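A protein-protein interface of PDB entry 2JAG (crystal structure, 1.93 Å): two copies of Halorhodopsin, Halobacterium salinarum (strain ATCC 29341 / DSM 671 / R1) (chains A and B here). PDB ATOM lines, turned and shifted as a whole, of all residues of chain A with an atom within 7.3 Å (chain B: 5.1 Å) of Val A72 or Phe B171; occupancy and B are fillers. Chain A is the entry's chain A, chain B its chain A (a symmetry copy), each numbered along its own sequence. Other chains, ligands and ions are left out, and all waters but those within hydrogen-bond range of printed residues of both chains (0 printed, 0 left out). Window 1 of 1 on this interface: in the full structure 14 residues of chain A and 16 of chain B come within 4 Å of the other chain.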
ATOM      1  N   ALA A  40      21.455  15.445 -25.805  1.00  0.00           N
ATOM      2  CA  ALA A  40      20.465  14.452 -25.383  1.00  0.00           C
ATOM      3  C   ALA A  40      19.094  14.798 -25.984  1.00  0.00           C
ATOM      4  O   ALA A  40      18.343  13.909 -26.402  1.00  0.00           O
ATOM      5  CB  ALA A  40      20.384  14.400 -23.856  1.00  0.00           C
ATOM      6  N   ILE A  44      16.858  12.376 -28.616  1.00  0.00           N
ATOM      7  CA  ILE A  44      15.468  11.968 -28.439  1.00  0.00           C
ATOM      8  C   ILE A  44      14.654  12.168 -29.718  1.00  0.00           C
ATOM      9  O   ILE A  44      13.912  11.274 -30.141  1.00  0.00           O
ATOM     10  CB  ILE A  44      14.821  12.756 -27.281  1.00  0.00           C
ATOM     11  CG1 ILE A  44      15.489  12.357 -25.963  1.00  0.00           C
ATOM     12  CG2 ILE A  44      13.321  12.497 -27.235  1.00  0.00           C
ATOM     13  CD1 ILE A  44      15.100  13.219 -24.778  1.00  0.00           C
ATOM     14  N   LEU A  67      14.782   4.911 -26.379  1.00  0.00           N
ATOM     15  CA  LEU A  67      14.357   6.297 -26.161  1.00  0.00           C
ATOM     16  C   LEU A  67      14.553   6.717 -24.702  1.00  0.00           C
ATOM     17  O   LEU A  67      14.784   7.889 -24.413  1.00  0.00           O
ATOM     18  CB  LEU A  67      12.870   6.474 -26.509  1.00  0.00           C
ATOM     19  CG  LEU A  67      12.379   6.256 -27.941  1.00  0.00           C
ATOM     20  CD1 LEU A  67      10.856   6.318 -27.964  1.00  0.00           C
ATOM     21  CD2 LEU A  67      12.968   7.312 -28.860  1.00  0.00           C
ATOM     22  N   MET A  68      14.438   5.750 -23.795  1.00  0.00           N
ATOM     23  CA  MET A  68      14.574   5.984 -22.355  1.00  0.00           C
ATOM     24  C   MET A  68      15.974   6.433 -21.942  1.00  0.00           C
ATOM     25  O   MET A  68      16.131   7.132 -20.946  1.00  0.00           O
ATOM     26  CB  MET A  68      14.241   4.703 -21.578  1.00  0.00           C
ATOM     27  CG  MET A  68      12.780   4.248 -21.607  1.00  0.00           C
ATOM     28  SD  MET A  68      11.745   5.035 -20.343  1.00  0.00           S
ATOM     29  CE  MET A  68      12.785   4.852 -18.887  1.00  0.00           C
ATOM     30  N   ILE A  69      16.986   6.012 -22.699  1.00  0.00           N
ATOM     31  CA  ILE A  69      18.371   6.347 -22.386  1.00  0.00           C
ATOM     32  C   ILE A  69      18.623   7.855 -22.392  1.00  0.00           C
ATOM     33  O   ILE A  69      19.110   8.410 -21.403  1.00  0.00           O
ATOM     34  CB  ILE A  69      19.337   5.611 -23.358  1.00  0.00           C
ATOM     35  CG1 ILE A  69      19.207   4.098 -23.133  1.00  0.00           C
ATOM     36  CG2 ILE A  69      20.775   6.088 -23.150  1.00  0.00           C
ATOM     37  CD1 ILE A  69      19.948   3.230 -24.142  1.00  0.00           C
ATOM     38  N   PRO A  70      18.299   8.545 -23.497  1.00  0.00           N
ATOM     39  CA  PRO A  70      18.534   9.992 -23.491  1.00  0.00           C
ATOM     40  C   PRO A  70      17.568  10.758 -22.560  1.00  0.00           C
ATOM     41  O   PRO A  70      17.905  11.830 -22.067  1.00  0.00           O
ATOM     42  CB  PRO A  70      18.385  10.374 -24.969  1.00  0.00           C
ATOM     43  CG  PRO A  70      17.434   9.335 -25.495  1.00  0.00           C
ATOM     44  CD  PRO A  70      17.943   8.075 -24.850  1.00  0.00           C
ATOM     45  N   LEU A  71      16.381  10.202 -22.315  1.00  0.00           N
ATOM     46  CA  LEU A  71      15.407  10.840 -21.423  1.00  0.00           C
ATOM     47  C   LEU A  71      15.956  10.863 -19.997  1.00  0.00           C
ATOM     48  O   LEU A  71      15.880  11.880 -19.299  1.00  0.00           O
ATOM     49  CB  LEU A  71      14.078  10.074 -21.436  1.00  0.00           C
ATOM     50  CG  LEU A  71      13.146  10.311 -22.623  1.00  0.00           C
ATOM     51  CD1 LEU A  71      12.046   9.260 -22.634  1.00  0.00           C
ATOM     52  CD2 LEU A  71      12.563  11.724 -22.531  1.00  0.00           C
ATOM     53  N   VAL A  72      16.496   9.726 -19.565  1.00  0.00           N
ATOM     54  CA  VAL A  72      17.081   9.617 -18.231  1.00  0.00           C
ATOM     55  C   VAL A  72      18.297  10.535 -18.161  1.00  0.00           C
ATOM     56  O   VAL A  72      18.487  11.264 -17.180  1.00  0.00           O
ATOM     57  CB  VAL A  72      17.501   8.160 -17.926  1.00  0.00           C
ATOM     58  CG1 VAL A  72      18.240   8.093 -16.582  1.00  0.00           C
ATOM     59  CG2 VAL A  72      16.260   7.262 -17.911  1.00  0.00           C
ATOM     60  N   SER A  73      19.115  10.512 -19.209  1.00  0.00           N
ATOM     61  CA  SER A  73      20.299  11.366 -19.262  1.00  0.00           C
ATOM     62  C   SER A  73      19.959  12.855 -19.089  1.00  0.00           C
ATOM     63  O   SER A  73      20.634  13.562 -18.341  1.00  0.00           O
ATOM     64  CB  SER A  73      21.042  11.168 -20.584  1.00  0.00           C
ATOM     65  OG  SER A  73      22.232  11.932 -20.599  1.00  0.00           O
ATOM     66  N   ILE A  74      18.929  13.337 -19.787  1.00  0.00           N
ATOM     67  CA  ILE A  74      18.534  14.743 -19.655  1.00  0.00           C
ATOM     68  C   ILE A  74      18.153  15.046 -18.207  1.00  0.00           C
ATOM     69  O   ILE A  74      18.525  16.085 -17.659  1.00  0.00           O
ATOM     70  CB  ILE A  74      17.332  15.106 -20.570  1.00  0.00           C
ATOM     71  CG1 ILE A  74      17.799  15.232 -22.016  1.00  0.00           C
ATOM     72  CG2 ILE A  74      16.707  16.426 -20.123  1.00  0.00           C
ATOM     73  CD1 ILE A  74      16.726  15.711 -22.986  1.00  0.00           C
ATOM     74  N   SER A  75      17.414  14.133 -17.586  1.00  0.00           N
ATOM     75  CA  SER A  75      17.008  14.304 -16.197  1.00  0.00           C
ATOM     76  C   SER A  75      18.247  14.450 -15.308  1.00  0.00           C
ATOM     77  O   SER A  75      18.269  15.261 -14.383  1.00  0.00           O
ATOM     78  CB  SER A  75      16.193  13.093 -15.731  1.00  0.00           C
ATOM     79  OG  SER A  75      15.055  12.882 -16.553  1.00  0.00           O
ATOM     80  N   SER A  76      19.276  13.660 -15.596  1.00  0.00           N
ATOM     81  CA  SER A  76      20.517  13.696 -14.820  1.00  0.00           C
ATOM     82  C   SER A  76      21.228  15.046 -14.922  1.00  0.00           C
ATOM     83  O   SER A  76      21.639  15.624 -13.912  1.00  0.00           O
ATOM     84  CB  SER A  76      21.467  12.581 -15.285  1.00  0.00           C
ATOM     85  OG  SER A  76      22.682  12.617 -14.554  1.00  0.00           O
ATOM     86  N   TYR A  77      21.369  15.559 -16.139  1.00  0.00           N
ATOM     87  CA  TYR A  77      22.030  16.837 -16.322  1.00  0.00           C
ATOM     88  C   TYR A  77      21.222  18.004 -15.743  1.00  0.00           C
ATOM     89  O   TYR A  77      21.793  19.019 -15.368  1.00  0.00           O
ATOM     90  CB  TYR A  77      22.345  17.049 -17.805  1.00  0.00           C
ATOM     91  CG  TYR A  77      23.559  16.252 -18.244  1.00  0.00           C
ATOM     92  CD1 TYR A  77      24.849  16.728 -18.004  1.00  0.00           C
ATOM     93  CD2 TYR A  77      23.419  14.993 -18.834  1.00  0.00           C
ATOM     94  CE1 TYR A  77      25.981  15.965 -18.337  1.00  0.00           C
ATOM     95  CE2 TYR A  77      24.543  14.222 -19.172  1.00  0.00           C
ATOM     96  CZ  TYR A  77      25.815  14.718 -18.919  1.00  0.00           C
ATOM     97  OH  TYR A  77      26.928  13.979 -19.258  1.00  0.00           O
ATOM     98  N   LEU A  78      19.902  17.854 -15.663  1.00  0.00           N
ATOM     99  CA  LEU A  78      19.072  18.908 -15.083  1.00  0.00           C
ATOM    100  C   LEU A  78      19.345  18.934 -13.579  1.00  0.00           C
ATOM    101  O   LEU A  78      19.442  20.002 -12.968  1.00  0.00           O
ATOM    102  CB  LEU A  78      17.583  18.636 -15.327  1.00  0.00           C
ATOM    103  CG  LEU A  78      17.038  18.788 -16.747  1.00  0.00           C
ATOM    104  CD1 LEU A  78      15.569  18.400 -16.771  1.00  0.00           C
ATOM    105  CD2 LEU A  78      17.216  20.222 -17.211  1.00  0.00           C
ATOM    106  N   THR A 111      21.961   8.698 -10.959  1.00  0.00           N
ATOM    107  CA  THR A 111      21.157   8.483 -12.158  1.00  0.00           C
ATOM    108  C   THR A 111      21.614   7.295 -13.014  1.00  0.00           C
ATOM    109  O   THR A 111      20.804   6.682 -13.716  1.00  0.00           O
ATOM    110  CB  THR A 111      21.105   9.763 -13.017  1.00  0.00           C
ATOM    111  OG1 THR A 111      20.725  10.877 -12.192  1.00  0.00           O
ATOM    112  CG2 THR A 111      20.078   9.612 -14.122  1.00  0.00           C
ATOM    113  N   TRP A 112      22.901   6.963 -12.951  1.00  0.00           N
ATOM    114  CA  TRP A 112      23.419   5.827 -13.710  1.00  0.00           C
ATOM    115  C   TRP A 112      22.653   4.576 -13.298  1.00  0.00           C
ATOM    116  O   TRP A 112      22.345   3.704 -14.128  1.00  0.00           O
ATOM    117  CB  TRP A 112      24.913   5.616 -13.443  1.00  0.00           C
ATOM    118  CG  TRP A 112      25.794   6.697 -14.001  1.00  0.00           C
ATOM    119  CD1 TRP A 112      25.521   7.517 -15.063  1.00  0.00           C
ATOM    120  CD2 TRP A 112      27.109   7.046 -13.555  1.00  0.00           C
ATOM    121  NE1 TRP A 112      26.585   8.355 -15.300  1.00  0.00           N
ATOM    122  CE2 TRP A 112      27.574   8.087 -14.389  1.00  0.00           C
ATOM    123  CE3 TRP A 112      27.941   6.579 -12.530  1.00  0.00           C
ATOM    124  CZ2 TRP A 112      28.839   8.670 -14.228  1.00  0.00           C
ATOM    125  CZ3 TRP A 112      29.204   7.162 -12.372  1.00  0.00           C
ATOM    126  CH2 TRP A 112      29.636   8.195 -13.217  1.00  0.00           C
ATOM    127  N   ALA A 113      22.359   4.483 -12.005  1.00  0.00           N
ATOM    128  CA  ALA A 113      21.595   3.348 -11.472  1.00  0.00           C
ATOM    129  C   ALA A 113      20.284   3.147 -12.226  1.00  0.00           C
ATOM    130  O   ALA A 113      19.624   2.118 -12.084  1.00  0.00           O
ATOM    131  CB  ALA A 113      21.319   3.543  -9.978  1.00  0.00           C
ATOM    132  N   LEU A 114      19.905   4.134 -13.031  1.00  0.00           N
ATOM    133  CA  LEU A 114      18.692   4.027 -13.829  1.00  0.00           C
ATOM    134  C   LEU A 114      19.044   3.938 -15.320  1.00  0.00           C
ATOM    135  O   LEU A 114      18.331   3.284 -16.076  1.00  0.00           O
ATOM    136  CB  LEU A 114      17.757   5.220 -13.587  1.00  0.00           C
ATOM    137  CG  LEU A 114      16.441   5.183 -14.381  1.00  0.00           C
ATOM    138  CD1 LEU A 114      15.646   3.936 -14.016  1.00  0.00           C
ATOM    139  CD2 LEU A 114      15.622   6.436 -14.088  1.00  0.00           C
ATOM    140  N   SER A 115      20.103   4.619 -15.735  1.00  0.00           N
ATOM    141  CA  SER A 115      20.489   4.558 -17.129  1.00  0.00           C
ATOM    142  C   SER A 115      21.273   3.294 -17.513  1.00  0.00           C
ATOM    143  O   SER A 115      21.025   2.765 -18.599  1.00  0.00           O
ATOM    144  CB  SER A 115      21.253   5.828 -17.539  1.00  0.00           C
ATOM    145  OG  SER A 115      22.011   6.361 -16.469  1.00  0.00           O
ATOM    146  N   THR A 116      22.183   2.786 -16.665  1.00  0.00           N
ATOM    147  CA  THR A 116      22.904   1.601 -17.053  1.00  0.00           C
ATOM    148  C   THR A 116      21.924   0.423 -17.189  1.00  0.00           C
ATOM    149  O   THR A 116      22.061  -0.391 -18.100  1.00  0.00           O
ATOM    150  CB  THR A 116      24.093   1.342 -16.118  1.00  0.00           C
ATOM    151  OG1 THR A 116      23.686   1.414 -14.754  1.00  0.00           O
ATOM    152  CG2 THR A 116      25.143   2.407 -16.357  1.00  0.00           C
ATOM    153  N   MET A 118      18.827   0.438 -18.269  1.00  0.00           N
ATOM    154  CA  MET A 118      18.090   0.530 -19.532  1.00  0.00           C
ATOM    155  C   MET A 118      18.981   0.160 -20.718  1.00  0.00           C
ATOM    156  O   MET A 118      18.511  -0.405 -21.710  1.00  0.00           O
ATOM    157  CB  MET A 118      17.504   1.934 -19.717  1.00  0.00           C
ATOM    158  CG  MET A 118      16.252   2.187 -18.873  1.00  0.00           C
ATOM    159  SD  MET A 118      14.884   1.059 -19.259  1.00  0.00           S
ATOM    160  CE  MET A 118      15.273  -0.324 -18.259  1.00  0.00           C
ATOM    161  N   LYS A 242      26.174   6.479 -24.441  1.00  0.00           N
ATOM    162  CA  LYS A 242      24.716   6.603 -24.485  1.00  0.00           C
ATOM    163  C   LYS A 242      24.123   6.963 -25.845  1.00  0.00           C
ATOM    164  O   LYS A 242      23.434   6.152 -26.459  1.00  0.00           O
ATOM    165  CB  LYS A 242      24.228   7.627 -23.455  1.00  0.00           C
ATOM    166  CG  LYS A 242      24.227   7.109 -22.029  1.00  0.00           C
ATOM    167  CD  LYS A 242      23.664   8.139 -21.047  1.00  0.00           C
ATOM    168  CE  LYS A 242      23.691   7.588 -19.629  1.00  0.00           C
ATOM    169  NZ  LYS A 242      24.942   6.881 -19.393  1.00  0.00           N
ATOM    170  N   ALA B 140       9.946   3.189 -17.028  1.00  0.00           N
ATOM    171  CA  ALA B 140       9.441   4.513 -17.384  1.00  0.00           C
ATOM    172  C   ALA B 140       8.604   5.085 -16.239  1.00  0.00           C
ATOM    173  O   ALA B 140       8.635   6.289 -15.968  1.00  0.00           O
ATOM    174  CB  ALA B 140       8.602   4.434 -18.668  1.00  0.00           C
ATOM    175  N   GLY B 143      10.875   6.373 -13.580  1.00  0.00           N
ATOM    176  CA  GLY B 143      11.451   7.637 -14.014  1.00  0.00           C
ATOM    177  C   GLY B 143      10.452   8.773 -13.847  1.00  0.00           C
ATOM    178  O   GLY B 143      10.818   9.886 -13.459  1.00  0.00           O
ATOM    179  N   MET B 144       9.183   8.490 -14.132  1.00  0.00           N
ATOM    180  CA  MET B 144       8.131   9.497 -13.993  1.00  0.00           C
ATOM    181  C   MET B 144       8.026   9.964 -12.540  1.00  0.00           C
ATOM    182  O   MET B 144       7.945  11.165 -12.265  1.00  0.00           O
ATOM    183  CB  MET B 144       6.775   8.923 -14.450  1.00  0.00           C
ATOM    184  CG  MET B 144       5.567   9.864 -14.233  1.00  0.00           C
ATOM    185  SD  MET B 144       3.959   9.068 -14.626  1.00  0.00           S
ATOM    186  CE  MET B 144       3.729   8.045 -13.174  1.00  0.00           C
ATOM    187  N   THR B 147      11.367  11.950 -11.293  1.00  0.00           N
ATOM    188  CA  THR B 147      11.551  13.285 -11.856  1.00  0.00           C
ATOM    189  C   THR B 147      10.471  14.206 -11.290  1.00  0.00           C
ATOM    190  O   THR B 147      10.652  15.421 -11.209  1.00  0.00           O
ATOM    191  CB  THR B 147      11.538  13.285 -13.420  1.00  0.00           C
ATOM    192  OG1 THR B 147      10.384  12.594 -13.916  1.00  0.00           O
ATOM    193  CG2 THR B 147      12.807  12.609 -13.951  1.00  0.00           C
ATOM    194  N   ILE B 167       9.707  16.600 -18.217  1.00  0.00           N
ATOM    195  CA  ILE B 167      10.358  15.317 -18.474  1.00  0.00           C
ATOM    196  C   ILE B 167       9.525  14.197 -17.857  1.00  0.00           C
ATOM    197  O   ILE B 167       9.408  13.109 -18.427  1.00  0.00           O
ATOM    198  CB  ILE B 167      11.785  15.266 -17.883  1.00  0.00           C
ATOM    199  CG1 ILE B 167      12.701  16.220 -18.648  1.00  0.00           C
ATOM    200  CG2 ILE B 167      12.349  13.855 -17.985  1.00  0.00           C
ATOM    201  CD1 ILE B 167      12.900  15.832 -20.109  1.00  0.00           C
ATOM    202  N   SER B 168       8.940  14.474 -16.693  1.00  0.00           N
ATOM    203  CA  SER B 168       8.106  13.487 -16.023  1.00  0.00           C
ATOM    204  C   SER B 168       6.919  13.167 -16.933  1.00  0.00           C
ATOM    205  O   SER B 168       6.510  12.013 -17.051  1.00  0.00           O
ATOM    206  CB  SER B 168       7.623  14.034 -14.682  1.00  0.00           C
ATOM    207  OG  SER B 168       6.901  13.049 -13.967  1.00  0.00           O
ATOM    208  N   CYS B 169       6.374  14.196 -17.580  1.00  0.00           N
ATOM    209  CA  CYS B 169       5.249  14.013 -18.498  1.00  0.00           C
ATOM    210  C   CYS B 169       5.640  13.086 -19.647  1.00  0.00           C
ATOM    211  O   CYS B 169       4.832  12.266 -20.093  1.00  0.00           O
ATOM    212  CB  CYS B 169       4.791  15.362 -19.067  1.00  0.00           C
ATOM    213  SG  CYS B 169       3.810  16.351 -17.917  1.00  0.00           S
ATOM    214  N   ALA B 170       6.876  13.225 -20.123  1.00  0.00           N
ATOM    215  CA  ALA B 170       7.383  12.394 -21.212  1.00  0.00           C
ATOM    216  C   ALA B 170       7.408  10.918 -20.814  1.00  0.00           C
ATOM    217  O   ALA B 170       7.030  10.050 -21.609  1.00  0.00           O
ATOM    218  CB  ALA B 170       8.779  12.856 -21.616  1.00  0.00           C
ATOM    219  N   PHE B 171       7.867  10.625 -19.597  1.00  0.00           N
ATOM    220  CA  PHE B 171       7.894   9.239 -19.119  1.00  0.00           C
ATOM    221  C   PHE B 171       6.450   8.733 -19.030  1.00  0.00           C
ATOM    222  O   PHE B 171       6.158   7.581 -19.355  1.00  0.00           O
ATOM    223  CB  PHE B 171       8.561   9.145 -17.733  1.00  0.00           C
ATOM    224  CG  PHE B 171      10.071   9.162 -17.770  1.00  0.00           C
ATOM    225  CD1 PHE B 171      10.779   8.160 -18.438  1.00  0.00           C
ATOM    226  CD2 PHE B 171      10.788  10.154 -17.103  1.00  0.00           C
ATOM    227  CE1 PHE B 171      12.186   8.148 -18.440  1.00  0.00           C
ATOM    228  CE2 PHE B 171      12.193  10.148 -17.100  1.00  0.00           C
ATOM    229  CZ  PHE B 171      12.890   9.141 -17.771  1.00  0.00           C
ATOM    230  N   PHE B 172       5.544   9.601 -18.588  1.00  0.00           N
ATOM    231  CA  PHE B 172       4.133   9.233 -18.476  1.00  0.00           C
ATOM    232  C   PHE B 172       3.609   8.780 -19.845  1.00  0.00           C
ATOM    233  O   PHE B 172       2.845   7.816 -19.945  1.00  0.00           O
ATOM    234  CB  PHE B 172       3.335  10.437 -17.943  1.00  0.00           C
ATOM    235  CG  PHE B 172       1.874  10.163 -17.695  1.00  0.00           C
ATOM    236  CD1 PHE B 172       1.438   8.916 -17.252  1.00  0.00           C
ATOM    237  CD2 PHE B 172       0.936  11.182 -17.844  1.00  0.00           C
ATOM    238  CE1 PHE B 172       0.089   8.687 -16.954  1.00  0.00           C
ATOM    239  CE2 PHE B 172      -0.419  10.968 -17.548  1.00  0.00           C
ATOM    240  CZ  PHE B 172      -0.840   9.717 -17.102  1.00  0.00           C
ATOM    241  N   VAL B 173       4.038   9.465 -20.902  1.00  0.00           N
ATOM    242  CA  VAL B 173       3.617   9.117 -22.259  1.00  0.00           C
ATOM    243  C   VAL B 173       4.140   7.734 -22.652  1.00  0.00           C
ATOM    244  O   VAL B 173       3.455   6.975 -23.335  1.00  0.00           O
ATOM    245  CB  VAL B 173       4.114  10.183 -23.270  1.00  0.00           C
ATOM    246  CG1 VAL B 173       3.855   9.732 -24.711  1.00  0.00           C
ATOM    247  CG2 VAL B 173       3.398  11.499 -23.002  1.00  0.00           C
ATOM    248  N   VAL B 174       5.353   7.401 -22.214  1.00  0.00           N
ATOM    249  CA  VAL B 174       5.918   6.092 -22.524  1.00  0.00           C
ATOM    250  C   VAL B 174       5.021   5.018 -21.906  1.00  0.00           C
ATOM    251  O   VAL B 174       4.670   4.042 -22.566  1.00  0.00           O
ATOM    252  CB  VAL B 174       7.365   5.945 -21.983  1.00  0.00           C
ATOM    253  CG1 VAL B 174       7.860   4.519 -22.189  1.00  0.00           C
ATOM    254  CG2 VAL B 174       8.292   6.915 -22.716  1.00  0.00           C
ATOM    255  N   VAL B 175       4.639   5.214 -20.646  1.00  0.00           N
ATOM    256  CA  VAL B 175       3.764   4.272 -19.952  1.00  0.00           C
ATOM    257  C   VAL B 175       2.416   4.118 -20.670  1.00  0.00           C
ATOM    258  O   VAL B 175       1.945   2.998 -20.903  1.00  0.00           O
ATOM    259  CB  VAL B 175       3.489   4.730 -18.501  1.00  0.00           C
ATOM    260  CG1 VAL B 175       2.464   3.807 -17.847  1.00  0.00           C
ATOM    261  CG2 VAL B 175       4.792   4.736 -17.695  1.00  0.00           C
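The backbone carbonyl oxygen of Gly B143 is in hydrogen-bond range of the side-chain hydroxyl of Thr B147.
The backbone carbonyl oxygen (O) of Met B144 is in hydrogen-bond range of the side-chain hydroxyl (OG1) of Thr B147 (3.3 Å).
The side-chain hydroxyl (OG) of Ser A75 is in hydrogen-bond range of the backbone carbonyl oxygen (O) of Leu A71.
Hydrophobic or aromatic side chains of chain A that line the printed part of chain B: Met A68, Leu A71, Val A72 and Ile A74.
Of the 13 printed residues of chain B, 4 touch a printed residue of chain A.
Hydrophobic or aromatic side chains of chain B that line the printed part of chain A: Ala B140, Ile B167 and Phe B171.
Among the printed residues, no Asp or Glu carboxylate lies within 4 Å of a Lys or Arg side-chain nitrogen of the other chain.
No position is printed for both chains.
Of the 8 pairs that touch across the chains among the printed residues, none has its exchanged pair printed and touching as well.
Of the printed residues of chain B, Val A72 touches Phe B171 (3.9 Å).
No residue of chain A comes within 4 Å of Ala B170.
Of the printed residues of chain A, Thr B147 touches Ser A75.
Of the printed residues of chain A, Ala B140 touches Met A68 (3.6 Å).
The nearest printed residue of chain B that does not touch Val A72 is Ile B167 (6.1 Å).
The nearest printed residue of chain A that does not touch Phe B171 is Leu A114 (5.3 Å).
Ala B140 touches Met A68.
Phe B171 touches Met A68.
Phe B171 touches Leu A71.
CG2 of Val A72 touches CZ of Phe B171, at 3.9 Å.
Ile A74 touches Ile B167 (CG2 to CD1, 3.9 Å).
Thr B147 touches Ser A75 (CG2 to OG, 3.4 Å).
CG2 of Ile B167 touches OG of Ser A75, at 3.2 Å.
Phe B171 touches Ser A75.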
